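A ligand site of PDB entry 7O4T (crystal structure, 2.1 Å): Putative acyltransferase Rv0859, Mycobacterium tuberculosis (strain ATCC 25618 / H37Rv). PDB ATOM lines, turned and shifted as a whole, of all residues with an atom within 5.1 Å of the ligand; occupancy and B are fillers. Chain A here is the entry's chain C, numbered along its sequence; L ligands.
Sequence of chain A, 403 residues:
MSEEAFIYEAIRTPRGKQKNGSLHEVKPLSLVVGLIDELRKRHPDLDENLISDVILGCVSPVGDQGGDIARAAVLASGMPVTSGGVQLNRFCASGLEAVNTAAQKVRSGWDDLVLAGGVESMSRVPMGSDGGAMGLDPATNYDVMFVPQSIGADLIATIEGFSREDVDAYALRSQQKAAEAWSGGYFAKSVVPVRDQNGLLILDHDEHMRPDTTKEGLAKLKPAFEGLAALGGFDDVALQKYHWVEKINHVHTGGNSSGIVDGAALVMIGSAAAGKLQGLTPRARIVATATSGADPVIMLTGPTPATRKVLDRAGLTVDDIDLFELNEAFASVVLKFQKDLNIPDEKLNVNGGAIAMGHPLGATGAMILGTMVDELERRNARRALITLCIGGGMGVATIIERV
A nitrogen (N6) of the ligand lies within hydrogen-bond range of the backbone carbonyl oxygen of Ser 258, 3.1 Å away. SG of Cys 92 lies close to S1 of the ligand (3.2 Å). The side-chain hydroxyl of Thr 213 is in hydrogen-bond range of a nitrogen (N3) of the ligand. NH1 of Arg 210 lies within salt-bridge range of O8 of the ligand, at 3.9 Å. The side-chain amide nitrogen (NE2) of Gln 149 sits close to a sulfur (S1) of the ligand, 3.2 Å away.
N of Ser 258 sits at hydrogen-bond distance from O of Ala 329. The backbone NH of Gln 18 sits close to the backbone carbonyl oxygen of Ile 260, at 3.3 Å. N of Arg 210 lies within hydrogen-bond range of OE1 of Gln 175 (3.0 Å). The side-chain hydroxyl of Thr 253 is in hydrogen-bond range of the backbone NH of Gly 255, at 3.0 Å. The backbone carbonyl oxygen (O) of Thr 253 sits at hydrogen-bond distance from the side-chain hydroxyl (OG) of Ser 257, 2.8 Å away. The side-chain hydroxyl of Thr 213 lies within hydrogen-bond range of the backbone carbonyl oxygen of Arg 210. The side-chain sulfur (SG) of Cys 92 is in hydrogen-bond range of the side-chain amide nitrogen (NE2) of Gln 149 (3.4 Å). O of Gly 259 is in hydrogen-bond range of N of His 359 (2.8 Å).
Met 127 touches the ligand (CE to O16, 3.9 Å). NE2 of Gln 175 touches N3 of the ligand, 3.8 Å away. CD2 of Leu 218 touches N3 of the ligand, 3.8 Å away. Leu 221 touches the ligand. CB of Ala 224 touches C14 of the ligand, 3.9 Å away. Phe 225 touches the ligand (CZ to C13, 3.4 Å). O of Thr 253 touches C13 of the ligand, at 3.7 Å. O of Gly 254 touches N4 of the ligand (3.5 Å). Gly 255 touches the ligand (CA to N4, 3.5 Å). CB of Ser 257 touches C13 of the ligand, at 3.99 Å. Ile 260 touches the ligand (CD1 to C16, 3.98 Å). Ala 329 touches the ligand (CB to S1, 3.6 Å). His 359 touches the ligand. 18 residues have an atom within 4 Å of the ligand: Cys 92, Met 127, Gln 149, Gln 175, Arg 210, Thr 213, Leu 218, Leu 221, Ala 224, Phe 225, Thr 253, Gly 254, Gly 255, Ser 257, Ser 258, Ile 260, Ala 329 and His 359. The nearest printed residue that does not touch the ligand is Leu 361 (4.01 Å).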
ATOM      1  N   GLN A  18      -2.984 -28.992 -12.350  1.00  0.00           N
ATOM      2  CA  GLN A  18      -3.287 -29.890 -13.456  1.00  0.00           C
ATOM      3  C   GLN A  18      -3.200 -29.180 -14.808  1.00  0.00           C
ATOM      4  O   GLN A  18      -2.591 -29.695 -15.755  1.00  0.00           O
ATOM      5  CB  GLN A  18      -4.671 -30.506 -13.275  1.00  0.00           C
ATOM      6  CG  GLN A  18      -5.058 -31.517 -14.336  1.00  0.00           C
ATOM      7  CD  GLN A  18      -6.520 -31.916 -14.281  1.00  0.00           C
ATOM      8  OE1 GLN A  18      -7.371 -31.130 -13.867  1.00  0.00           O
ATOM      9  NE2 GLN A  18      -6.808 -33.146 -14.676  1.00  0.00           N
ATOM     10  N   LYS A  19      -3.805 -27.994 -14.909  1.00  0.00           N
ATOM     11  CA  LYS A  19      -3.821 -27.234 -16.155  1.00  0.00           C
ATOM     12  C   LYS A  19      -2.661 -26.247 -16.159  1.00  0.00           C
ATOM     13  O   LYS A  19      -2.571 -25.381 -15.292  1.00  0.00           O
ATOM     14  CB  LYS A  19      -5.150 -26.486 -16.310  1.00  0.00           C
ATOM     15  CG  LYS A  19      -6.174 -27.191 -17.193  1.00  0.00           C
ATOM     16  CD  LYS A  19      -6.714 -28.455 -16.530  1.00  0.00           C
ATOM     17  CE  LYS A  19      -7.808 -29.073 -17.377  1.00  0.00           C
ATOM     18  NZ  LYS A  19      -8.378 -30.296 -16.753  1.00  0.00           N
ATOM     19  N   CYS A  92      -6.763 -43.270  -1.614  1.00  0.00           N
ATOM     20  CA  CYS A  92      -6.357 -41.937  -1.159  1.00  0.00           C
ATOM     21  C   CYS A  92      -5.403 -41.993   0.039  1.00  0.00           C
ATOM     22  O   CYS A  92      -4.609 -41.065   0.235  1.00  0.00           O
ATOM     23  CB  CYS A  92      -7.592 -41.107  -0.802  1.00  0.00           C
ATOM     24  SG  CYS A  92      -8.806 -40.982  -2.134  1.00  0.00           S
ATOM     25  N   MET A 127      -6.199 -39.970 -13.024  1.00  0.00           N
ATOM     26  CA  MET A 127      -6.894 -40.893 -12.138  1.00  0.00           C
ATOM     27  C   MET A 127      -7.728 -41.872 -12.951  1.00  0.00           C
ATOM     28  O   MET A 127      -8.433 -41.488 -13.887  1.00  0.00           O
ATOM     29  CB  MET A 127      -7.778 -40.109 -11.166  1.00  0.00           C
ATOM     30  CG  MET A 127      -8.592 -40.949 -10.207  1.00  0.00           C
ATOM     31  SD  MET A 127      -9.361 -39.932  -8.938  1.00  0.00           S
ATOM     32  CE  MET A 127     -10.004 -38.577  -9.928  1.00  0.00           C
ATOM     33  N   GLN A 149     -16.678 -40.907  -6.177  1.00  0.00           N
ATOM     34  CA  GLN A 149     -16.575 -40.284  -4.860  1.00  0.00           C
ATOM     35  C   GLN A 149     -17.387 -39.007  -4.761  1.00  0.00           C
ATOM     36  O   GLN A 149     -17.878 -38.665  -3.676  1.00  0.00           O
ATOM     37  CB  GLN A 149     -15.106 -39.985  -4.543  1.00  0.00           C
ATOM     38  CG  GLN A 149     -14.323 -41.164  -3.996  1.00  0.00           C
ATOM     39  CD  GLN A 149     -12.843 -41.047  -4.264  1.00  0.00           C
ATOM     40  OE1 GLN A 149     -12.423 -40.658  -5.351  1.00  0.00           O
ATOM     41  NE2 GLN A 149     -12.028 -41.396  -3.268  1.00  0.00           N
ATOM     42  N   GLN A 175      -8.592 -21.906   1.986  1.00  0.00           N
ATOM     43  CA  GLN A 175      -7.748 -20.974   1.242  1.00  0.00           C
ATOM     44  C   GLN A 175      -7.070 -19.976   2.174  1.00  0.00           C
ATOM     45  O   GLN A 175      -5.870 -19.720   2.074  1.00  0.00           O
ATOM     46  CB  GLN A 175      -8.567 -20.246   0.185  1.00  0.00           C
ATOM     47  CG  GLN A 175      -9.188 -21.141  -0.882  1.00  0.00           C
ATOM     48  CD  GLN A 175      -8.200 -21.556  -1.952  1.00  0.00           C
ATOM     49  OE1 GLN A 175      -7.006 -21.266  -1.872  1.00  0.00           O
ATOM     50  NE2 GLN A 175      -8.703 -22.236  -2.982  1.00  0.00           N
ATOM     51  N   ARG A 210      -5.505 -20.317  -4.302  1.00  0.00           N
ATOM     52  CA  ARG A 210      -6.160 -19.078  -4.725  1.00  0.00           C
ATOM     53  C   ARG A 210      -6.407 -18.245  -3.484  1.00  0.00           C
ATOM     54  O   ARG A 210      -7.531 -18.188  -2.965  1.00  0.00           O
ATOM     55  CB  ARG A 210      -7.460 -19.366  -5.476  1.00  0.00           C
ATOM     56  CG  ARG A 210      -7.273 -20.007  -6.851  1.00  0.00           C
ATOM     57  CD  ARG A 210      -8.621 -20.339  -7.478  1.00  0.00           C
ATOM     58  NE  ARG A 210      -8.552 -20.432  -8.929  1.00  0.00           N
ATOM     59  CZ  ARG A 210      -8.400 -21.569  -9.611  1.00  0.00           C
ATOM     60  NH1 ARG A 210      -8.309 -22.724  -8.965  1.00  0.00           N
ATOM     61  NH2 ARG A 210      -8.351 -21.545 -10.937  1.00  0.00           N
ATOM     62  N   THR A 213      -9.527 -15.794  -2.808  1.00  0.00           N
ATOM     63  CA  THR A 213     -10.869 -16.339  -2.939  1.00  0.00           C
ATOM     64  C   THR A 213     -11.847 -15.556  -2.066  1.00  0.00           C
ATOM     65  O   THR A 213     -11.506 -15.119  -0.959  1.00  0.00           O
ATOM     66  CB  THR A 213     -10.879 -17.816  -2.556  1.00  0.00           C
ATOM     67  OG1 THR A 213      -9.922 -18.524  -3.362  1.00  0.00           O
ATOM     68  CG2 THR A 213     -12.245 -18.435  -2.777  1.00  0.00           C
ATOM     69  N   GLY A 217     -17.169 -15.183  -5.189  1.00  0.00           N
ATOM     70  CA  GLY A 217     -16.589 -15.956  -6.286  1.00  0.00           C
ATOM     71  C   GLY A 217     -16.928 -17.425  -6.200  1.00  0.00           C
ATOM     72  O   GLY A 217     -17.209 -18.066  -7.216  1.00  0.00           O
ATOM     73  N   LEU A 218     -16.911 -17.986  -4.983  1.00  0.00           N
ATOM     74  CA  LEU A 218     -17.278 -19.387  -4.810  1.00  0.00           C
ATOM     75  C   LEU A 218     -18.737 -19.632  -5.161  1.00  0.00           C
ATOM     76  O   LEU A 218     -19.074 -20.700  -5.685  1.00  0.00           O
ATOM     77  CB  LEU A 218     -16.993 -19.837  -3.380  1.00  0.00           C
ATOM     78  CG  LEU A 218     -15.518 -19.982  -2.994  1.00  0.00           C
ATOM     79  CD1 LEU A 218     -15.373 -20.235  -1.500  1.00  0.00           C
ATOM     80  CD2 LEU A 218     -14.861 -21.098  -3.781  1.00  0.00           C
ATOM     81  N   LEU A 221     -19.596 -20.437  -9.006  1.00  0.00           N
ATOM     82  CA  LEU A 221     -19.174 -21.669  -9.673  1.00  0.00           C
ATOM     83  C   LEU A 221     -20.347 -22.615  -9.876  1.00  0.00           C
ATOM     84  O   LEU A 221     -21.334 -22.582  -9.135  1.00  0.00           O
ATOM     85  CB  LEU A 221     -18.072 -22.357  -8.858  1.00  0.00           C
ATOM     86  CG  LEU A 221     -16.898 -21.453  -8.458  1.00  0.00           C
ATOM     87  CD1 LEU A 221     -15.792 -22.255  -7.806  1.00  0.00           C
ATOM     88  CD2 LEU A 221     -16.374 -20.670  -9.659  1.00  0.00           C
ATOM     89  N   ALA A 224     -19.849 -29.141 -10.219  1.00  0.00           N
ATOM     90  CA  ALA A 224     -18.971 -29.839 -11.145  1.00  0.00           C
ATOM     91  C   ALA A 224     -19.359 -31.287 -11.386  1.00  0.00           C
ATOM     92  O   ALA A 224     -18.816 -31.908 -12.299  1.00  0.00           O
ATOM     93  CB  ALA A 224     -17.527 -29.775 -10.627  1.00  0.00           C
ATOM     94  N   PHE A 225     -20.284 -31.834 -10.607  1.00  0.00           N
ATOM     95  CA  PHE A 225     -20.574 -33.263 -10.634  1.00  0.00           C
ATOM     96  C   PHE A 225     -22.037 -33.569 -10.913  1.00  0.00           C
ATOM     97  O   PHE A 225     -22.507 -34.671 -10.592  1.00  0.00           O
ATOM     98  CB  PHE A 225     -20.112 -33.916  -9.337  1.00  0.00           C
ATOM     99  CG  PHE A 225     -18.663 -33.715  -9.043  1.00  0.00           C
ATOM    100  CD1 PHE A 225     -17.693 -34.285  -9.870  1.00  0.00           C
ATOM    101  CD2 PHE A 225     -18.253 -32.971  -7.958  1.00  0.00           C
ATOM    102  CE1 PHE A 225     -16.357 -34.106  -9.604  1.00  0.00           C
ATOM    103  CE2 PHE A 225     -16.907 -32.788  -7.693  1.00  0.00           C
ATOM    104  CZ  PHE A 225     -15.956 -33.365  -8.518  1.00  0.00           C
ATOM    105  N   THR A 253     -18.089 -28.176  -6.054  1.00  0.00           N
ATOM    106  CA  THR A 253     -17.592 -27.530  -7.264  1.00  0.00           C
ATOM    107  C   THR A 253     -16.083 -27.651  -7.330  1.00  0.00           C
ATOM    108  O   THR A 253     -15.470 -28.306  -6.486  1.00  0.00           O
ATOM    109  CB  THR A 253     -17.989 -26.043  -7.286  1.00  0.00           C
ATOM    110  OG1 THR A 253     -17.283 -25.361  -6.246  1.00  0.00           O
ATOM    111  CG2 THR A 253     -19.490 -25.870  -7.048  1.00  0.00           C
ATOM    112  N   GLY A 254     -15.460 -26.999  -8.322  1.00  0.00           N
ATOM    113  CA  GLY A 254     -14.017 -26.888  -8.319  1.00  0.00           C
ATOM    114  C   GLY A 254     -13.462 -26.010  -7.224  1.00  0.00           C
ATOM    115  O   GLY A 254     -12.258 -26.058  -6.964  1.00  0.00           O
ATOM    116  N   GLY A 255     -14.303 -25.220  -6.565  1.00  0.00           N
ATOM    117  CA  GLY A 255     -13.853 -24.326  -5.513  1.00  0.00           C
ATOM    118  C   GLY A 255     -13.891 -24.929  -4.130  1.00  0.00           C
ATOM    119  O   GLY A 255     -13.213 -24.444  -3.221  1.00  0.00           O
ATOM    120  N   SER A 257     -13.829 -28.564  -3.725  1.00  0.00           N
ATOM    121  CA  SER A 257     -13.318 -29.922  -3.822  1.00  0.00           C
ATOM    122  C   SER A 257     -11.797 -29.893  -3.865  1.00  0.00           C
ATOM    123  O   SER A 257     -11.192 -28.866  -4.177  1.00  0.00           O
ATOM    124  CB  SER A 257     -13.871 -30.637  -5.065  1.00  0.00           C
ATOM    125  OG  SER A 257     -15.278 -30.696  -5.054  1.00  0.00           O
ATOM    126  N   SER A 258     -11.190 -31.027  -3.550  1.00  0.00           N
ATOM    127  CA  SER A 258      -9.740 -31.128  -3.604  1.00  0.00           C
ATOM    128  C   SER A 258      -9.244 -30.889  -5.024  1.00  0.00           C
ATOM    129  O   SER A 258      -9.908 -31.257  -6.008  1.00  0.00           O
ATOM    130  CB  SER A 258      -9.276 -32.500  -3.112  1.00  0.00           C
ATOM    131  OG  SER A 258      -9.714 -33.527  -3.983  1.00  0.00           O
ATOM    132  N   GLY A 259      -8.076 -30.277  -5.132  1.00  0.00           N
ATOM    133  CA  GLY A 259      -7.491 -30.021  -6.440  1.00  0.00           C
ATOM    134  C   GLY A 259      -6.718 -31.210  -6.959  1.00  0.00           C
ATOM    135  O   GLY A 259      -6.156 -32.013  -6.204  1.00  0.00           O
ATOM    136  N   ILE A 260      -6.689 -31.335  -8.276  1.00  0.00           N
ATOM    137  CA  ILE A 260      -5.923 -32.371  -8.963  1.00  0.00           C
ATOM    138  C   ILE A 260      -4.530 -31.807  -9.237  1.00  0.00           C
ATOM    139  O   ILE A 260      -4.375 -30.866 -10.007  1.00  0.00           O
ATOM    140  CB  ILE A 260      -6.616 -32.799 -10.261  1.00  0.00           C
ATOM    141  CG1 ILE A 260      -7.957 -33.471  -9.951  1.00  0.00           C
ATOM    142  CG2 ILE A 260      -5.713 -33.716 -11.083  1.00  0.00           C
ATOM    143  CD1 ILE A 260      -8.781 -33.809 -11.173  1.00  0.00           C
ATOM    144  N   LEU A 300     -17.190 -42.117   1.491  1.00  0.00           N
ATOM    145  CA  LEU A 300     -16.355 -41.099   2.126  1.00  0.00           C
ATOM    146  C   LEU A 300     -16.667 -40.912   3.609  1.00  0.00           C
ATOM    147  O   LEU A 300     -16.394 -39.838   4.154  1.00  0.00           O
ATOM    148  CB  LEU A 300     -16.493 -39.777   1.381  1.00  0.00           C
ATOM    149  CG  LEU A 300     -16.072 -39.790  -0.089  1.00  0.00           C
ATOM    150  CD1 LEU A 300     -16.423 -38.481  -0.762  1.00  0.00           C
ATOM    151  CD2 LEU A 300     -14.584 -40.077  -0.220  1.00  0.00           C
ATOM    152  N   ALA A 329     -10.722 -33.913   0.750  1.00  0.00           N
ATOM    153  CA  ALA A 329     -11.182 -34.450  -0.529  1.00  0.00           C
ATOM    154  C   ALA A 329     -12.397 -33.694  -1.039  1.00  0.00           C
ATOM    155  O   ALA A 329     -12.465 -33.303  -2.204  1.00  0.00           O
ATOM    156  CB  ALA A 329     -11.487 -35.941  -0.390  1.00  0.00           C
ATOM    157  N   PHE A 330     -13.375 -33.473  -0.156  1.00  0.00           N
ATOM    158  CA  PHE A 330     -14.515 -32.626  -0.426  1.00  0.00           C
ATOM    159  C   PHE A 330     -14.895 -31.914   0.867  1.00  0.00           C
ATOM    160  O   PHE A 330     -14.599 -32.396   1.962  1.00  0.00           O
ATOM    161  CB  PHE A 330     -15.715 -33.409  -0.977  1.00  0.00           C
ATOM    162  CG  PHE A 330     -15.418 -34.153  -2.252  1.00  0.00           C
ATOM    163  CD1 PHE A 330     -15.614 -33.542  -3.484  1.00  0.00           C
ATOM    164  CD2 PHE A 330     -14.949 -35.453  -2.231  1.00  0.00           C
ATOM    165  CE1 PHE A 330     -15.336 -34.206  -4.661  1.00  0.00           C
ATOM    166  CE2 PHE A 330     -14.667 -36.128  -3.400  1.00  0.00           C
ATOM    167  CZ  PHE A 330     -14.864 -35.510  -4.621  1.00  0.00           C
ATOM    168  N   HIS A 359      -4.569 -32.336  -3.927  1.00  0.00           N
ATOM    169  CA  HIS A 359      -4.652 -33.694  -3.411  1.00  0.00           C
ATOM    170  C   HIS A 359      -3.940 -34.647  -4.363  1.00  0.00           C
ATOM    171  O   HIS A 359      -4.585 -35.323  -5.186  1.00  0.00           O
ATOM    172  CB  HIS A 359      -6.110 -34.092  -3.202  1.00  0.00           C
ATOM    173  CG  HIS A 359      -6.308 -35.500  -2.738  1.00  0.00           C
ATOM    174  ND1 HIS A 359      -5.302 -36.253  -2.165  1.00  0.00           N
ATOM    175  CD2 HIS A 359      -7.409 -36.300  -2.753  1.00  0.00           C
ATOM    176  CE1 HIS A 359      -5.771 -37.450  -1.851  1.00  0.00           C
ATOM    177  NE2 HIS A 359      -7.046 -37.494  -2.196  1.00  0.00           N
ATOM    178  N   LEU A 361      -3.038 -37.785  -4.937  1.00  0.00           N
ATOM    179  CA  LEU A 361      -3.513 -39.048  -4.376  1.00  0.00           C
ATOM    180  C   LEU A 361      -2.495 -39.830  -3.553  1.00  0.00           C
ATOM    181  O   LEU A 361      -2.561 -39.828  -2.323  1.00  0.00           O
ATOM    182  CB  LEU A 361      -4.032 -39.948  -5.511  1.00  0.00           C
ATOM    183  CG  LEU A 361      -5.123 -39.340  -6.392  1.00  0.00           C
ATOM    184  CD1 LEU A 361      -5.663 -40.377  -7.372  1.00  0.00           C
ATOM    185  CD2 LEU A 361      -6.249 -38.748  -5.559  1.00  0.00           C
ATOM    186  N   CYS A 389     -10.136 -40.037   4.160  1.00  0.00           N
ATOM    187  CA  CYS A 389     -11.136 -40.862   3.521  1.00  0.00           C
ATOM    188  C   CYS A 389     -10.507 -41.588   2.331  1.00  0.00           C
ATOM    189  O   CYS A 389      -9.490 -41.178   1.782  1.00  0.00           O
ATOM    190  CB  CYS A 389     -12.328 -40.012   3.054  1.00  0.00           C
ATOM    191  SG  CYS A 389     -11.890 -38.580   2.055  1.00  0.00           S
HETATM  192  N1  LIG L   1     -12.197 -19.140  -6.560  1.00  0.00           N
HETATM  193  C1  LIG L   1     -12.677 -18.734  -7.742  1.00  0.00           C
HETATM  194  N2  LIG L   1     -12.882 -19.434  -8.861  1.00  0.00           N
HETATM  195  C2  LIG L   1     -12.521 -20.720  -8.678  1.00  0.00           C
HETATM  196  C3  LIG L   1     -12.020 -21.283  -7.535  1.00  0.00           C
HETATM  197  C4  LIG L   1     -11.854 -20.445  -6.418  1.00  0.00           C
HETATM  198  N3  LIG L   1     -11.375 -20.850  -5.246  1.00  0.00           N
HETATM  199  N4  LIG L   1     -11.774 -22.644  -7.736  1.00  0.00           N
HETATM  200  C5  LIG L   1     -12.124 -22.858  -8.989  1.00  0.00           C
HETATM  201  N5  LIG L   1     -12.587 -21.728  -9.603  1.00  0.00           N
HETATM  202  C6  LIG L   1     -13.064 -21.590 -10.983  1.00  0.00           C
HETATM  203  C7  LIG L   1     -12.036 -21.938 -12.048  1.00  0.00           C
HETATM  204  O1  LIG L   1     -11.198 -20.857 -12.397  1.00  0.00           O
HETATM  205  C8  LIG L   1     -12.941 -22.443 -13.172  1.00  0.00           C
HETATM  206  O2  LIG L   1     -13.617 -21.344 -13.779  1.00  0.00           O
HETATM  207  P1  LIG L   1     -13.716 -21.603 -15.375  1.00  0.00           P
HETATM  208  O3  LIG L   1     -12.278 -21.610 -15.883  1.00  0.00           O
HETATM  209  O4  LIG L   1     -14.399 -22.932 -15.582  1.00  0.00           O
HETATM  210  O5  LIG L   1     -14.515 -20.446 -15.943  1.00  0.00           O
HETATM  211  C9  LIG L   1     -13.908 -23.282 -12.353  1.00  0.00           C
HETATM  212  O6  LIG L   1     -14.151 -22.477 -11.179  1.00  0.00           O
HETATM  213  C10 LIG L   1     -13.311 -24.590 -11.902  1.00  0.00           C
HETATM  214  O7  LIG L   1     -12.377 -25.047 -12.909  1.00  0.00           O
HETATM  215  P2  LIG L   1     -11.009 -25.732 -12.431  1.00  0.00           P
HETATM  216  O8  LIG L   1     -10.578 -25.111 -11.144  1.00  0.00           O
HETATM  217  O9  LIG L   1     -10.034 -25.715 -13.572  1.00  0.00           O
HETATM  218  O10 LIG L   1     -11.479 -27.240 -12.178  1.00  0.00           O
HETATM  219  P3  LIG L   1     -12.116 -28.314 -13.190  1.00  0.00           P
HETATM  220  O11 LIG L   1     -13.449 -27.837 -13.646  1.00  0.00           O
HETATM  221  O12 LIG L   1     -11.087 -28.683 -14.208  1.00  0.00           O
HETATM  222  O13 LIG L   1     -12.322 -29.565 -12.217  1.00  0.00           O
HETATM  223  C11 LIG L   1     -13.318 -30.766 -10.367  1.00  0.00           C
HETATM  224  C12 LIG L   1     -13.078 -29.397 -10.988  1.00  0.00           C
HETATM  225  C13 LIG L   1     -14.066 -30.595  -9.046  1.00  0.00           C
HETATM  226  C14 LIG L   1     -14.191 -31.586 -11.333  1.00  0.00           C
HETATM  227  C15 LIG L   1     -11.996 -31.503 -10.127  1.00  0.00           C
HETATM  228  O14 LIG L   1     -11.118 -30.621  -9.439  1.00  0.00           O
HETATM  229  C16 LIG L   1     -12.153 -32.787  -9.321  1.00  0.00           C
HETATM  230  O15 LIG L   1     -12.741 -33.742  -9.809  1.00  0.00           O
HETATM  231  N6  LIG L   1     -11.614 -32.814  -8.106  1.00  0.00           N
HETATM  232  C17 LIG L   1     -12.002 -33.788  -7.100  1.00  0.00           C
HETATM  233  C18 LIG L   1     -11.016 -34.933  -6.989  1.00  0.00           C
HETATM  234  C19 LIG L   1     -11.736 -36.259  -7.118  1.00  0.00           C
HETATM  235  O16 LIG L   1     -12.616 -36.405  -7.971  1.00  0.00           O
HETATM  236  N7  LIG L   1     -11.387 -37.256  -6.301  1.00  0.00           N
HETATM  237  C20 LIG L   1     -10.359 -37.150  -5.282  1.00  0.00           C
HETATM  238  C21 LIG L   1     -10.120 -38.463  -4.572  1.00  0.00           C
HETATM  239  S1  LIG L   1     -10.689 -38.479  -2.848  1.00  0.00           S
